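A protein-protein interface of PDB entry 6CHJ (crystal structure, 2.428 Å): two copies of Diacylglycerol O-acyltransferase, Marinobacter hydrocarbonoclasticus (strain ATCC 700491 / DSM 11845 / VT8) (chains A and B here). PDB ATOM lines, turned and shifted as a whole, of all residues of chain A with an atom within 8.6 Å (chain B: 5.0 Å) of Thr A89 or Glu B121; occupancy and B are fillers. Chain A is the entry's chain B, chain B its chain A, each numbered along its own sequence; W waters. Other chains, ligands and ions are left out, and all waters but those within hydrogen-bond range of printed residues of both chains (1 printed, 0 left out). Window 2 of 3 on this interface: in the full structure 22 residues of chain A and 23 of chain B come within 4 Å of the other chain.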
ATOM      1  N   ALA A  86      22.360  14.616  -3.379  1.00  0.00           N
ATOM      2  CA  ALA A  86      21.453  15.377  -2.551  1.00  0.00           C
ATOM      3  C   ALA A  86      20.108  14.681  -2.524  1.00  0.00           C
ATOM      4  O   ALA A  86      19.709  14.035  -3.498  1.00  0.00           O
ATOM      5  CB  ALA A  86      21.272  16.804  -3.082  1.00  0.00           C
ATOM      6  N   LEU A  87      19.396  14.825  -1.362  1.00  0.00           N
ATOM      7  CA  LEU A  87      18.102  14.178  -1.305  1.00  0.00           C
ATOM      8  C   LEU A  87      17.038  15.100  -1.877  1.00  0.00           C
ATOM      9  O   LEU A  87      17.142  16.317  -1.761  1.00  0.00           O
ATOM     10  CB  LEU A  87      17.748  13.824   0.136  1.00  0.00           C
ATOM     11  CG  LEU A  87      18.585  12.734   0.806  1.00  0.00           C
ATOM     12  CD1 LEU A  87      18.035  12.510   2.171  1.00  0.00           C
ATOM     13  CD2 LEU A  87      18.599  11.421  -0.004  1.00  0.00           C
ATOM     14  N   PRO A  88      16.004  14.562  -2.503  1.00  0.00           N
ATOM     15  CA  PRO A  88      14.890  15.415  -2.928  1.00  0.00           C
ATOM     16  C   PRO A  88      14.090  15.883  -1.717  1.00  0.00           C
ATOM     17  O   PRO A  88      14.058  15.226  -0.672  1.00  0.00           O
ATOM     18  CB  PRO A  88      14.057  14.487  -3.816  1.00  0.00           C
ATOM     19  CG  PRO A  88      14.271  13.121  -3.186  1.00  0.00           C
ATOM     20  CD  PRO A  88      15.684  13.123  -2.614  1.00  0.00           C
ATOM     21  N   THR A  89      13.444  17.043  -1.875  1.00  0.00           N
ATOM     22  CA  THR A  89      12.520  17.549  -0.866  1.00  0.00           C
ATOM     23  C   THR A  89      11.529  16.445  -0.481  1.00  0.00           C
ATOM     24  O   THR A  89      10.927  15.823  -1.370  1.00  0.00           O
ATOM     25  CB  THR A  89      11.770  18.780  -1.403  1.00  0.00           C
ATOM     26  OG1 THR A  89      12.682  19.874  -1.548  1.00  0.00           O
ATOM     27  CG2 THR A  89      10.648  19.209  -0.466  1.00  0.00           C
ATOM     28  N   PRO A  90      11.300  16.196   0.823  1.00  0.00           N
ATOM     29  CA  PRO A  90      11.734  17.026   1.957  1.00  0.00           C
ATOM     30  C   PRO A  90      12.967  16.560   2.722  1.00  0.00           C
ATOM     31  O   PRO A  90      13.145  16.991   3.865  1.00  0.00           O
ATOM     32  CB  PRO A  90      10.507  17.000   2.882  1.00  0.00           C
ATOM     33  CG  PRO A  90       9.717  15.729   2.479  1.00  0.00           C
ATOM     34  CD  PRO A  90      10.367  15.138   1.246  1.00  0.00           C
ATOM     35  N   GLY A  91      13.787  15.699   2.125  1.00  0.00           N
ATOM     36  CA  GLY A  91      15.086  15.396   2.701  1.00  0.00           C
ATOM     37  C   GLY A  91      15.090  14.659   4.026  1.00  0.00           C
ATOM     38  O   GLY A  91      16.081  14.727   4.762  1.00  0.00           O
ATOM     39  N   ARG A  92      14.032  13.940   4.352  1.00  0.00           N
ATOM     40  CA  ARG A  92      13.983  13.235   5.626  1.00  0.00           C
ATOM     41  C   ARG A  92      14.312  11.750   5.425  1.00  0.00           C
ATOM     42  O   ARG A  92      14.802  11.325   4.368  1.00  0.00           O
ATOM     43  CB  ARG A  92      12.619  13.439   6.285  1.00  0.00           C
ATOM     44  CG  ARG A  92      11.527  12.697   5.589  1.00  0.00           C
ATOM     45  CD  ARG A  92      10.172  13.360   5.748  1.00  0.00           C
ATOM     46  NE  ARG A  92       9.263  12.919   4.692  1.00  0.00           N
ATOM     47  CZ  ARG A  92       8.708  11.715   4.639  1.00  0.00           C
ATOM     48  NH1 ARG A  92       8.961  10.811   5.593  1.00  0.00           N
ATOM     49  NH2 ARG A  92       7.898  11.411   3.631  1.00  0.00           N
ATOM     50  N   GLU A  95      13.302   9.653   2.426  1.00  0.00           N
ATOM     51  CA  GLU A  95      14.065   9.920   1.202  1.00  0.00           C
ATOM     52  C   GLU A  95      15.478   9.322   1.267  1.00  0.00           C
ATOM     53  O   GLU A  95      15.969   8.767   0.273  1.00  0.00           O
ATOM     54  CB  GLU A  95      14.117  11.427   0.915  1.00  0.00           C
ATOM     55  CG  GLU A  95      12.799  12.007   0.375  1.00  0.00           C
ATOM     56  CD  GLU A  95      11.677  12.017   1.419  1.00  0.00           C
ATOM     57  OE1 GLU A  95      10.563  11.507   1.146  1.00  0.00           O
ATOM     58  OE2 GLU A  95      11.923  12.537   2.529  1.00  0.00           O
ATOM     59  N   GLU A 121      23.847  15.156   0.789  1.00  0.00           N
ATOM     60  CA  GLU A 121      23.405  16.393   1.415  1.00  0.00           C
ATOM     61  C   GLU A 121      21.892  16.480   1.271  1.00  0.00           C
ATOM     62  O   GLU A 121      21.242  15.560   0.769  1.00  0.00           O
ATOM     63  CB  GLU A 121      24.106  17.624   0.798  1.00  0.00           C
ATOM     64  CG  GLU A 121      23.517  18.122  -0.549  1.00  0.00           C
ATOM     65  CD  GLU A 121      23.841  19.611  -0.865  1.00  0.00           C
ATOM     66  OE1 GLU A 121      24.832  20.150  -0.329  1.00  0.00           O
ATOM     67  OE2 GLU A 121      23.111  20.238  -1.677  1.00  0.00           O
ATOM     68  N   GLY A 122      21.325  17.591   1.745  1.00  0.00           N
ATOM     69  CA  GLY A 122      19.889  17.791   1.714  1.00  0.00           C
ATOM     70  C   GLY A 122      19.107  17.123   2.826  1.00  0.00           C
ATOM     71  O   GLY A 122      17.878  17.064   2.745  1.00  0.00           O
ATOM     72  N   LEU A 123      19.763  16.601   3.854  1.00  0.00           N
ATOM     73  CA  LEU A 123      19.008  16.051   4.971  1.00  0.00           C
ATOM     74  C   LEU A 123      18.508  17.193   5.854  1.00  0.00           C
ATOM     75  O   LEU A 123      19.127  18.256   5.930  1.00  0.00           O
ATOM     76  CB  LEU A 123      19.862  15.063   5.763  1.00  0.00           C
ATOM     77  CG  LEU A 123      19.937  13.665   5.120  1.00  0.00           C
ATOM     78  CD1 LEU A 123      20.965  13.582   3.967  1.00  0.00           C
ATOM     79  CD2 LEU A 123      20.203  12.602   6.162  1.00  0.00           C
ATOM     80  N   LYS A 124      17.365  16.972   6.504  1.00  0.00           N
ATOM     81  CA  LYS A 124      16.622  18.045   7.157  1.00  0.00           C
ATOM     82  C   LYS A 124      17.421  18.825   8.196  1.00  0.00           C
ATOM     83  O   LYS A 124      17.869  19.942   7.917  1.00  0.00           O
ATOM     84  CB  LYS A 124      15.340  17.497   7.793  1.00  0.00           C
ATOM     85  CG  LYS A 124      14.107  18.053   7.101  1.00  0.00           C
ATOM     86  CD  LYS A 124      12.785  17.504   7.620  1.00  0.00           C
ATOM     87  CE  LYS A 124      11.609  18.267   6.962  1.00  0.00           C
ATOM     88  NZ  LYS A 124      10.322  17.487   6.881  1.00  0.00           N
ATOM     89  N   VAL B  40       8.457  21.921  -8.101  1.00  0.00           N
ATOM     90  CA  VAL B  40       8.845  20.584  -8.557  1.00  0.00           C
ATOM     91  C   VAL B  40       8.395  19.525  -7.553  1.00  0.00           C
ATOM     92  O   VAL B  40       7.882  18.457  -7.941  1.00  0.00           O
ATOM     93  CB  VAL B  40      10.360  20.493  -8.844  1.00  0.00           C
ATOM     94  CG1 VAL B  40      10.626  19.313  -9.763  1.00  0.00           C
ATOM     95  CG2 VAL B  40      10.884  21.780  -9.487  1.00  0.00           C
ATOM     96  N   ALA B  41       8.558  19.802  -6.248  1.00  0.00           N
ATOM     97  CA  ALA B  41       8.027  18.883  -5.240  1.00  0.00           C
ATOM     98  C   ALA B  41       6.518  18.695  -5.405  1.00  0.00           C
ATOM     99  O   ALA B  41       6.012  17.564  -5.345  1.00  0.00           O
ATOM    100  CB  ALA B  41       8.372  19.373  -3.838  1.00  0.00           C
ATOM    101  N   PHE B  84      12.049  10.861  -8.205  1.00  0.00           N
ATOM    102  CA  PHE B  84      12.127  12.281  -7.904  1.00  0.00           C
ATOM    103  C   PHE B  84      13.421  12.501  -7.143  1.00  0.00           C
ATOM    104  O   PHE B  84      13.615  11.942  -6.059  1.00  0.00           O
ATOM    105  CB  PHE B  84      10.920  12.733  -7.072  1.00  0.00           C
ATOM    106  CG  PHE B  84      10.947  14.195  -6.668  1.00  0.00           C
ATOM    107  CD1 PHE B  84      11.165  15.179  -7.604  1.00  0.00           C
ATOM    108  CD2 PHE B  84      10.710  14.574  -5.359  1.00  0.00           C
ATOM    109  CE1 PHE B  84      11.165  16.525  -7.244  1.00  0.00           C
ATOM    110  CE2 PHE B  84      10.707  15.914  -4.994  1.00  0.00           C
ATOM    111  CZ  PHE B  84      10.944  16.895  -5.949  1.00  0.00           C
ATOM    112  N   GLU B  85      14.308  13.306  -7.714  1.00  0.00           N
ATOM    113  CA  GLU B  85      15.689  13.373  -7.272  1.00  0.00           C
ATOM    114  C   GLU B  85      16.150  14.816  -7.363  1.00  0.00           C
ATOM    115  O   GLU B  85      15.485  15.675  -7.960  1.00  0.00           O
ATOM    116  CB  GLU B  85      16.576  12.408  -8.102  1.00  0.00           C
ATOM    117  CG  GLU B  85      15.923  10.991  -8.259  1.00  0.00           C
ATOM    118  CD  GLU B  85      16.534  10.079  -9.336  1.00  0.00           C
ATOM    119  OE1 GLU B  85      16.591  10.475 -10.515  1.00  0.00           O
ATOM    120  OE2 GLU B  85      16.897   8.926  -9.015  1.00  0.00           O
ATOM    121  N   ALA B  86      17.306  15.085  -6.766  1.00  0.00           N
ATOM    122  CA  ALA B  86      17.739  16.456  -6.604  1.00  0.00           C
ATOM    123  C   ALA B  86      19.234  16.548  -6.855  1.00  0.00           C
ATOM    124  O   ALA B  86      19.996  15.623  -6.549  1.00  0.00           O
ATOM    125  CB  ALA B  86      17.407  16.998  -5.197  1.00  0.00           C
ATOM    126  N   LEU B  87      19.634  17.699  -7.417  1.00  0.00           N
ATOM    127  CA  LEU B  87      21.010  18.092  -7.662  1.00  0.00           C
ATOM    128  C   LEU B  87      21.658  18.566  -6.367  1.00  0.00           C
ATOM    129  O   LEU B  87      21.028  19.281  -5.576  1.00  0.00           O
ATOM    130  CB  LEU B  87      21.083  19.219  -8.705  1.00  0.00           C
ATOM    131  CG  LEU B  87      20.749  18.879 -10.155  1.00  0.00           C
ATOM    132  CD1 LEU B  87      21.432  19.882 -11.066  1.00  0.00           C
ATOM    133  CD2 LEU B  87      21.184  17.435 -10.488  1.00  0.00           C
ATOM    134  N   LEU B 119      12.553  12.980 -12.489  1.00  0.00           N
ATOM    135  CA  LEU B 119      12.319  14.400 -12.285  1.00  0.00           C
ATOM    136  C   LEU B 119      13.393  14.929 -11.348  1.00  0.00           C
ATOM    137  O   LEU B 119      13.625  14.365 -10.275  1.00  0.00           O
ATOM    138  CB  LEU B 119      10.922  14.645 -11.711  1.00  0.00           C
ATOM    139  CG  LEU B 119      10.396  16.076 -11.504  1.00  0.00           C
ATOM    140  CD1 LEU B 119      10.098  16.775 -12.802  1.00  0.00           C
ATOM    141  CD2 LEU B 119       9.125  16.087 -10.610  1.00  0.00           C
ATOM    142  N   ILE B 120      14.072  15.992 -11.765  1.00  0.00           N
ATOM    143  CA  ILE B 120      15.229  16.515 -11.044  1.00  0.00           C
ATOM    144  C   ILE B 120      14.910  17.935 -10.567  1.00  0.00           C
ATOM    145  O   ILE B 120      14.629  18.828 -11.379  1.00  0.00           O
ATOM    146  CB  ILE B 120      16.491  16.488 -11.922  1.00  0.00           C
ATOM    147  CG1 ILE B 120      16.759  15.050 -12.445  1.00  0.00           C
ATOM    148  CG2 ILE B 120      17.674  17.078 -11.170  1.00  0.00           C
ATOM    149  CD1 ILE B 120      17.382  15.005 -13.839  1.00  0.00           C
ATOM    150  N   GLU B 121      14.941  18.137  -9.254  1.00  0.00           N
ATOM    151  CA  GLU B 121      14.851  19.470  -8.675  1.00  0.00           C
ATOM    152  C   GLU B 121      16.246  19.930  -8.264  1.00  0.00           C
ATOM    153  O   GLU B 121      17.251  19.243  -8.494  1.00  0.00           O
ATOM    154  CB  GLU B 121      13.891  19.499  -7.479  1.00  0.00           C
ATOM    155  CG  GLU B 121      14.448  18.807  -6.217  1.00  0.00           C
ATOM    156  CD  GLU B 121      13.752  19.243  -4.924  1.00  0.00           C
ATOM    157  OE1 GLU B 121      12.622  19.774  -5.010  1.00  0.00           O
ATOM    158  OE2 GLU B 121      14.339  19.063  -3.825  1.00  0.00           O
ATOM    159  N   GLY B 122      16.303  21.113  -7.645  1.00  0.00           N
ATOM    160  CA  GLY B 122      17.558  21.705  -7.232  1.00  0.00           C
ATOM    161  C   GLY B 122      18.342  22.412  -8.312  1.00  0.00           C
ATOM    162  O   GLY B 122      19.507  22.754  -8.071  1.00  0.00           O
ATOM    163  N   LEU B 123      17.765  22.627  -9.498  1.00  0.00           N
ATOM    164  CA  LEU B 123      18.402  23.507 -10.480  1.00  0.00           C
ATOM    165  C   LEU B 123      18.419  24.937  -9.963  1.00  0.00           C
ATOM    166  O   LEU B 123      17.544  25.350  -9.196  1.00  0.00           O
ATOM    167  CB  LEU B 123      17.677  23.474 -11.827  1.00  0.00           C
ATOM    168  CG  LEU B 123      17.523  22.158 -12.590  1.00  0.00           C
ATOM    169  CD1 LEU B 123      17.087  22.388 -14.034  1.00  0.00           C
ATOM    170  CD2 LEU B 123      18.820  21.427 -12.551  1.00  0.00           C
HETATM  171  O   HOH W   1      18.475  12.650  -5.704  1.00  0.00           O
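The backbone carbonyl oxygen (O) of Ala B86 sits close to the backbone carbonyl oxygen (O) of Ala A86, 3.5 Å away. The side-chain carboxylate (OE2) of Glu B121 is in hydrogen-bond range of the side-chain hydroxyl (OG1) of Thr A89, 2.9 Å away.
Along chain A the printed residues that touch a printed residue of chain B span positions 86 to 89. Of the 11 printed residues of chain B, 5 touch a printed residue of chain A. Printed residues of chain B that touch a printed residue of chain A: Phe B84, Glu B85, Ala B86, Leu B87 and Glu B121. Among the printed residues, 9 pairs touch across the chains. Among the printed residues, no Asp or Glu carboxylate lies within 4 Å of a Lys or Arg side-chain nitrogen of the other chain.
Ala B86 touches its own counterpart, Ala A86. Ala A86 touches Leu B87, and with the chains exchanged Leu A87 touches Ala B86. Positions printed for both chains: 86, 87, 121, 122 and 123. Of the 9 pairs that touch across the chains among the printed residues, 3 have their exchanged pair printed and touching as well.
Thr A89 touches just these residues of chain B: Phe B84 and Glu B121. Of chain A, only Pro A88 (3.8 Å) and Thr A89 (2.9 Å) come within 4 Å of Glu B121. Printed residues of chain B within 4 Å of Pro A88: Phe B84, Glu B85, Ala B86 and Glu B121. Of the printed residues of chain B, Leu A87 touches Ala B86 (3.5 Å). Of the printed residues of chain A, Ala B86 touches Ala A86 (3.5 Å), Leu A87 (3.5 Å) and Pro A88 (3.7 Å). Glu A121 touches none of the printed residues of chain B.
Water W1 lies within hydrogen-bond range of O of Ala A86 and N of Ala B86.
Among the printed residues, pairs that only touch across the chains: Pro A88 with Phe B84 (3.2 Å), Leu A87 with Ala B86 (3.5 Å), Ala A86 with Leu B87 (3.5 Å), Thr A89 with Phe B84 (3.6 Å), Pro A88 with Ala B86 (3.7 Å), Pro A88 with Glu B121 (3.8 Å) and Pro A88 with Glu B85 (3.98 Å).
The backbone carbonyl oxygen of Glu B85 is in hydrogen-bond range of the backbone NH of Glu B121. The backbone carbonyl oxygen (O) of Leu B119 sits at hydrogen-bond distance from the backbone NH (N) of Glu B85 (2.9 Å). The backbone carbonyl oxygen (O) of Glu B121 lies within hydrogen-bond range of the backbone NH (N) of Leu B87 (3.0 Å). The backbone NH (N) of Leu A87 lies within hydrogen-bond range of the backbone carbonyl oxygen (O) of Glu A121 (2.9 Å).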
